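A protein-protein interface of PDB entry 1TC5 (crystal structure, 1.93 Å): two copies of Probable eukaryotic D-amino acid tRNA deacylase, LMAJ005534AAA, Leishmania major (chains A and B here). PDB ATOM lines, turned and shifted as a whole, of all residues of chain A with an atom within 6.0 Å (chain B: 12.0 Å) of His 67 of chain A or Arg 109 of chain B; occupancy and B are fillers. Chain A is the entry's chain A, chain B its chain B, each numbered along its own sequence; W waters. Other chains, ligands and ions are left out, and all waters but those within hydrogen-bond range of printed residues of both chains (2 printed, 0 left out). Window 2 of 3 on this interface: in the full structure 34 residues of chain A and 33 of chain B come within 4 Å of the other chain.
N of Lys 69 of chain A sits at hydrogen-bond distance from O of Arg 109 of chain B (2.9 Å).
ND1 of His 67 of chain A lies close to O of Gly 63 of chain A. The backbone carbonyl oxygen (O) of Val 64 of chain A is in hydrogen-bond range of the side-chain hydroxyl (OG1) of Thr 68 of chain A (2.6 Å). The side-chain carboxylate of Glu 87 of chain A sits close to a ring nitrogen (NE2) of His 67 of chain A (3.4 Å). O of Lys 107 of chain B sits at hydrogen-bond distance from OG of Ser 110 of chain B, at 2.9 Å.
Among the printed residues, pairs that only touch across the chains: Val 64 of chain A with Val 106 of chain B, His 67 of chain A with Arg 109 of chain B, Thr 68 of chain A with Arg 109 of chain B, Thr 68 of chain A with Ser 110 of chain B, Lys 69 of chain A with Val 111 of chain B and Ile 70 of chain A with Val 111 of chain B.
No residue of chain B comes within 4 Å of Gly 63 of chain A. Printed residues of chain B within 4 Å of Val 64 of chain A: Val 106 (3.8 Å). Leu 65 of chain A touches none of the printed residues of chain B. His 67 of chain A touches one residue of chain B. Thr 68 of chain A touches just these residues of chain B: Arg 109 and Ser 110. Printed residues of chain B within 4 Å of Lys 69 of chain A: Arg 109 (2.9 Å) and Val 111 (3.8 Å). Of the printed residues of chain B, Ile 70 of chain A touches Val 111. No residue of chain B comes within 4 Å of Ser 85 of chain A. Printed residues of chain A within 4 Å of Arg 109 of chain B: His 67 (3.8 Å), Thr 68 (3.6 Å) and Lys 69 (2.9 Å). Of the printed residues of chain A, Val 111 of chain B touches Lys 69 and Ile 70. Gln 112 of chain B touches none of the printed residues of chain A. The nearest residue of chain B that does not touch His 67 of chain A is Ser 110 of chain B (5.8 Å).
Of the 10 printed residues of chain B, 4 touch a printed residue of chain A. Among the printed residues, 7 pairs touch across the chains. Among the printed residues, no Asp or Glu carboxylate lies within 4 Å of a Lys or Arg side-chain nitrogen of the other chain.
No position is printed for both chains. Of the 7 pairs that touch across the chains among the printed residues, none has its exchanged pair printed and touching as well.
Water W1 lies within hydrogen-bond range of the side-chain hydroxyl of Thr 68 of chain A (2.6 Å) and the backbone carbonyl oxygen of Gly 108 of chain B (2.6 Å). Water W2 lies within hydrogen-bond range of the backbone carbonyl oxygen (O) of Lys 69 of chain A (2.6 Å) and the backbone NH (N) of Val 111 of chain B (2.9 Å).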
ATOM      1  N   VAL A  62      14.337  32.389   8.305  1.00  0.00           N
ATOM      2  CA  VAL A  62      15.503  32.860   7.560  1.00  0.00           C
ATOM      3  C   VAL A  62      15.967  31.710   6.652  1.00  0.00           C
ATOM      4  O   VAL A  62      16.345  31.936   5.519  1.00  0.00           O
ATOM      5  CB  VAL A  62      16.643  33.332   8.495  1.00  0.00           C
ATOM      6  CG1 VAL A  62      17.944  33.576   7.706  1.00  0.00           C
ATOM      7  CG2 VAL A  62      16.259  34.594   9.220  1.00  0.00           C
ATOM      8  N   GLY A  63      15.907  30.485   7.158  1.00  0.00           N
ATOM      9  CA  GLY A  63      16.258  29.309   6.381  1.00  0.00           C
ATOM     10  C   GLY A  63      15.387  29.138   5.156  1.00  0.00           C
ATOM     11  O   GLY A  63      15.871  28.772   4.089  1.00  0.00           O
ATOM     12  N   VAL A  64      14.094  29.414   5.298  1.00  0.00           N
ATOM     13  CA  VAL A  64      13.188  29.355   4.152  1.00  0.00           C
ATOM     14  C   VAL A  64      13.586  30.410   3.122  1.00  0.00           C
ATOM     15  O   VAL A  64      13.689  30.128   1.935  1.00  0.00           O
ATOM     16  CB  VAL A  64      11.704  29.560   4.568  1.00  0.00           C
ATOM     17  CG1 VAL A  64      10.787  29.791   3.330  1.00  0.00           C
ATOM     18  CG2 VAL A  64      11.207  28.376   5.406  1.00  0.00           C
ATOM     19  N   LEU A  65      13.831  31.628   3.589  1.00  0.00           N
ATOM     20  CA  LEU A  65      14.317  32.691   2.719  1.00  0.00           C
ATOM     21  C   LEU A  65      15.609  32.341   1.970  1.00  0.00           C
ATOM     22  O   LEU A  65      15.731  32.643   0.795  1.00  0.00           O
ATOM     23  CB  LEU A  65      14.533  33.982   3.517  1.00  0.00           C
ATOM     24  CG  LEU A  65      15.153  35.148   2.733  1.00  0.00           C
ATOM     25  CD1 LEU A  65      14.218  35.616   1.587  1.00  0.00           C
ATOM     26  CD2 LEU A  65      15.449  36.298   3.657  1.00  0.00           C
ATOM     27  N   LEU A  66      16.569  31.710   2.643  1.00  0.00           N
ATOM     28  CA  LEU A  66      17.892  31.487   2.057  1.00  0.00           C
ATOM     29  C   LEU A  66      18.080  30.136   1.376  1.00  0.00           C
ATOM     30  O   LEU A  66      18.847  30.046   0.423  1.00  0.00           O
ATOM     31  CB  LEU A  66      18.987  31.710   3.114  1.00  0.00           C
ATOM     32  CG  LEU A  66      18.991  33.079   3.787  1.00  0.00           C
ATOM     33  CD1 LEU A  66      20.153  33.154   4.804  1.00  0.00           C
ATOM     34  CD2 LEU A  66      19.061  34.234   2.793  1.00  0.00           C
ATOM     35  N   HIS A  67      17.386  29.095   1.850  1.00  0.00           N
ATOM     36  CA  HIS A  67      17.580  27.719   1.363  1.00  0.00           C
ATOM     37  C   HIS A  67      16.681  27.346   0.196  1.00  0.00           C
ATOM     38  O   HIS A  67      16.957  26.402  -0.535  1.00  0.00           O
ATOM     39  CB  HIS A  67      17.313  26.679   2.480  1.00  0.00           C
ATOM     40  CG  HIS A  67      18.198  26.834   3.677  1.00  0.00           C
ATOM     41  ND1 HIS A  67      17.778  26.551   4.962  1.00  0.00           N
ATOM     42  CD2 HIS A  67      19.485  27.242   3.781  1.00  0.00           C
ATOM     43  CE1 HIS A  67      18.764  26.798   5.807  1.00  0.00           C
ATOM     44  NE2 HIS A  67      19.812  27.214   5.117  1.00  0.00           N
ATOM     45  N   THR A  68      15.561  28.024   0.066  1.00  0.00           N
ATOM     46  CA  THR A  68      14.606  27.701  -0.989  1.00  0.00           C
ATOM     47  C   THR A  68      15.133  28.215  -2.329  1.00  0.00           C
ATOM     48  O   THR A  68      15.596  29.344  -2.415  1.00  0.00           O
ATOM     49  CB  THR A  68      13.226  28.337  -0.666  1.00  0.00           C
ATOM     50  OG1 THR A  68      12.854  27.987   0.681  1.00  0.00           O
ATOM     51  CG2 THR A  68      12.110  27.759  -1.550  1.00  0.00           C
ATOM     52  N   LYS A  69      15.083  27.363  -3.348  1.00  0.00           N
ATOM     53  CA  LYS A  69      15.441  27.759  -4.703  1.00  0.00           C
ATOM     54  C   LYS A  69      14.241  28.462  -5.288  1.00  0.00           C
ATOM     55  O   LYS A  69      13.240  27.838  -5.562  1.00  0.00           O
ATOM     56  CB  LYS A  69      15.827  26.545  -5.529  1.00  0.00           C
ATOM     57  CG  LYS A  69      17.055  25.790  -4.960  1.00  0.00           C
ATOM     58  CD  LYS A  69      17.331  24.485  -5.734  1.00  0.00           C
ATOM     59  CE  LYS A  69      18.494  23.690  -5.138  1.00  0.00           C
ATOM     60  NZ  LYS A  69      19.768  23.859  -5.890  1.00  0.00           N
ATOM     61  N   ILE A  70      14.331  29.779  -5.431  1.00  0.00           N
ATOM     62  CA  ILE A  70      13.196  30.585  -5.860  1.00  0.00           C
ATOM     63  C   ILE A  70      13.472  31.264  -7.185  1.00  0.00           C
ATOM     64  O   ILE A  70      12.734  31.066  -8.131  1.00  0.00           O
ATOM     65  CB  ILE A  70      12.862  31.656  -4.785  1.00  0.00           C
ATOM     66  CG1 ILE A  70      12.572  30.984  -3.438  1.00  0.00           C
ATOM     67  CG2 ILE A  70      11.654  32.500  -5.233  1.00  0.00           C
ATOM     68  CD1 ILE A  70      12.697  31.942  -2.236  1.00  0.00           C
ATOM     69  N   SER A  85      18.929  29.037  -4.809  1.00  0.00           N
ATOM     70  CA  SER A  85      18.806  29.597  -3.480  1.00  0.00           C
ATOM     71  C   SER A  85      19.790  30.750  -3.296  1.00  0.00           C
ATOM     72  O   SER A  85      20.840  30.809  -3.929  1.00  0.00           O
ATOM     73  CB  SER A  85      19.097  28.536  -2.421  1.00  0.00           C
ATOM     74  OG  SER A  85      20.422  28.105  -2.520  1.00  0.00           O
ATOM     75  N   LEU A  86      19.429  31.676  -2.422  1.00  0.00           N
ATOM     76  CA  LEU A  86      20.366  32.684  -1.984  1.00  0.00           C
ATOM     77  C   LEU A  86      21.578  32.020  -1.363  1.00  0.00           C
ATOM     78  O   LEU A  86      22.693  32.486  -1.552  1.00  0.00           O
ATOM     79  CB  LEU A  86      19.715  33.629  -0.970  1.00  0.00           C
ATOM     80  CG  LEU A  86      18.895  34.704  -1.650  1.00  0.00           C
ATOM     81  CD1 LEU A  86      17.809  35.216  -0.703  1.00  0.00           C
ATOM     82  CD2 LEU A  86      19.840  35.845  -2.143  1.00  0.00           C
ATOM     83  N   GLU A  87      21.368  30.914  -0.646  1.00  0.00           N
ATOM     84  CA  GLU A  87      22.463  30.219   0.023  1.00  0.00           C
ATOM     85  C   GLU A  87      23.559  29.818  -0.974  1.00  0.00           C
ATOM     86  O   GLU A  87      24.730  30.042  -0.728  1.00  0.00           O
ATOM     87  CB  GLU A  87      21.934  29.005   0.809  1.00  0.00           C
ATOM     88  CG  GLU A  87      22.998  28.136   1.477  1.00  0.00           C
ATOM     89  CD  GLU A  87      22.408  26.915   2.181  1.00  0.00           C
ATOM     90  OE1 GLU A  87      21.646  26.144   1.543  1.00  0.00           O
ATOM     91  OE2 GLU A  87      22.701  26.721   3.394  1.00  0.00           O
ATOM     92  N   GLY B 104       2.737  30.743  -5.771  1.00  0.00           N
ATOM     93  CA  GLY B 104       3.781  29.804  -5.383  1.00  0.00           C
ATOM     94  C   GLY B 104       3.798  29.516  -3.879  1.00  0.00           C
ATOM     95  O   GLY B 104       3.522  30.413  -3.060  1.00  0.00           O
ATOM     96  N   LYS B 105       4.044  28.253  -3.538  1.00  0.00           N
ATOM     97  CA  LYS B 105       4.294  27.838  -2.162  1.00  0.00           C
ATOM     98  C   LYS B 105       5.584  27.018  -2.049  1.00  0.00           C
ATOM     99  O   LYS B 105       5.957  26.302  -2.965  1.00  0.00           O
ATOM    100  CB  LYS B 105       3.107  27.035  -1.625  1.00  0.00           C
ATOM    101  CG  LYS B 105       1.821  27.821  -1.594  1.00  0.00           C
ATOM    102  CD  LYS B 105       0.941  27.412  -0.432  1.00  0.00           C
ATOM    103  CE  LYS B 105      -0.325  26.695  -0.836  1.00  0.00           C
ATOM    104  NZ  LYS B 105      -0.635  25.582   0.129  1.00  0.00           N
ATOM    105  N   VAL B 106       6.255  27.146  -0.910  1.00  0.00           N
ATOM    106  CA  VAL B 106       7.426  26.348  -0.583  1.00  0.00           C
ATOM    107  C   VAL B 106       7.083  24.863  -0.468  1.00  0.00           C
ATOM    108  O   VAL B 106       6.118  24.483   0.222  1.00  0.00           O
ATOM    109  CB  VAL B 106       8.034  26.825   0.774  1.00  0.00           C
ATOM    110  CG1 VAL B 106       9.151  25.880   1.208  1.00  0.00           C
ATOM    111  CG2 VAL B 106       8.527  28.283   0.646  1.00  0.00           C
ATOM    112  N   LYS B 107       7.898  24.045  -1.125  1.00  0.00           N
ATOM    113  CA  LYS B 107       7.836  22.597  -1.080  1.00  0.00           C
ATOM    114  C   LYS B 107       9.278  22.108  -0.918  1.00  0.00           C
ATOM    115  O   LYS B 107      10.059  22.146  -1.879  1.00  0.00           O
ATOM    116  CB  LYS B 107       7.218  22.089  -2.389  1.00  0.00           C
ATOM    117  CG  LYS B 107       7.424  20.613  -2.734  1.00  0.00           C
ATOM    118  CD  LYS B 107       6.674  20.250  -4.032  1.00  0.00           C
ATOM    119  CE  LYS B 107       7.451  19.266  -4.876  1.00  0.00           C
ATOM    120  NZ  LYS B 107       7.853  18.088  -4.062  1.00  0.00           N
ATOM    121  N   GLY B 108       9.621  21.686   0.301  1.00  0.00           N
ATOM    122  CA  GLY B 108      10.990  21.334   0.652  1.00  0.00           C
ATOM    123  C   GLY B 108      11.876  22.541   0.432  1.00  0.00           C
ATOM    124  O   GLY B 108      11.650  23.584   1.046  1.00  0.00           O
ATOM    125  N   ARG B 109      12.817  22.419  -0.507  1.00  0.00           N
ATOM    126  CA  ARG B 109      13.714  23.519  -0.866  1.00  0.00           C
ATOM    127  C   ARG B 109      13.429  24.074  -2.261  1.00  0.00           C
ATOM    128  O   ARG B 109      14.278  24.641  -2.901  1.00  0.00           O
ATOM    129  CB  ARG B 109      15.168  23.056  -0.693  1.00  0.00           C
ATOM    130  CG  ARG B 109      15.511  22.843   0.796  1.00  0.00           C
ATOM    131  CD  ARG B 109      16.876  22.236   1.072  1.00  0.00           C
ATOM    132  NE  ARG B 109      17.210  21.146   0.147  1.00  0.00           N
ATOM    133  CZ  ARG B 109      17.002  19.841   0.364  1.00  0.00           C
ATOM    134  NH1 ARG B 109      16.447  19.397   1.494  1.00  0.00           N
ATOM    135  NH2 ARG B 109      17.373  18.962  -0.566  1.00  0.00           N
ATOM    136  N   SER B 110      12.201  23.903  -2.728  1.00  0.00           N
ATOM    137  CA  SER B 110      11.786  24.437  -4.005  1.00  0.00           C
ATOM    138  C   SER B 110      10.430  25.128  -3.861  1.00  0.00           C
ATOM    139  O   SER B 110       9.878  25.227  -2.757  1.00  0.00           O
ATOM    140  CB  SER B 110      11.718  23.308  -5.040  1.00  0.00           C
ATOM    141  OG  SER B 110      10.703  22.387  -4.720  1.00  0.00           O
ATOM    142  N   VAL B 111       9.910  25.608  -4.982  1.00  0.00           N
ATOM    143  CA  VAL B 111       8.610  26.260  -5.050  1.00  0.00           C
ATOM    144  C   VAL B 111       7.702  25.449  -5.996  1.00  0.00           C
ATOM    145  O   VAL B 111       8.113  25.061  -7.093  1.00  0.00           O
ATOM    146  CB  VAL B 111       8.689  27.751  -5.576  1.00  0.00           C
ATOM    147  CG1 VAL B 111       7.331  28.383  -5.664  1.00  0.00           C
ATOM    148  CG2 VAL B 111       9.631  28.604  -4.733  1.00  0.00           C
ATOM    149  N   GLN B 112       6.471  25.188  -5.544  1.00  0.00           N
ATOM    150  CA  GLN B 112       5.459  24.561  -6.382  1.00  0.00           C
ATOM    151  C   GLN B 112       4.376  25.579  -6.700  1.00  0.00           C
ATOM    152  O   GLN B 112       4.015  26.432  -5.869  1.00  0.00           O
ATOM    153  CB  GLN B 112       4.846  23.275  -5.782  1.00  0.00           C
ATOM    154  CG  GLN B 112       4.221  23.375  -4.355  1.00  0.00           C
ATOM    155  CD  GLN B 112       2.764  23.890  -4.297  1.00  0.00           C
ATOM    156  OE1 GLN B 112       2.149  24.219  -5.318  1.00  0.00           O
ATOM    157  NE2 GLN B 112       2.221  23.955  -3.083  1.00  0.00           N
ATOM    158  N   PHE B 113       3.850  25.467  -7.918  1.00  0.00           N
ATOM    159  CA  PHE B 113       2.881  26.397  -8.455  1.00  0.00           C
ATOM    160  C   PHE B 113       1.518  25.751  -8.747  1.00  0.00           C
ATOM    161  O   PHE B 113       0.771  26.208  -9.614  1.00  0.00           O
ATOM    162  CB  PHE B 113       3.437  27.028  -9.726  1.00  0.00           C
ATOM    163  CG  PHE B 113       4.612  27.947  -9.473  1.00  0.00           C
ATOM    164  CD1 PHE B 113       4.434  29.154  -8.785  1.00  0.00           C
ATOM    165  CD2 PHE B 113       5.891  27.589  -9.882  1.00  0.00           C
ATOM    166  CE1 PHE B 113       5.484  30.003  -8.554  1.00  0.00           C
ATOM    167  CE2 PHE B 113       6.986  28.439  -9.639  1.00  0.00           C
ATOM    168  CZ  PHE B 113       6.790  29.642  -8.973  1.00  0.00           C
HETATM  169  O   HOH W   1      12.969  25.709   1.884  1.00  0.00           O
HETATM  170  O   HOH W   2      11.934  26.143  -7.025  1.00  0.00           O
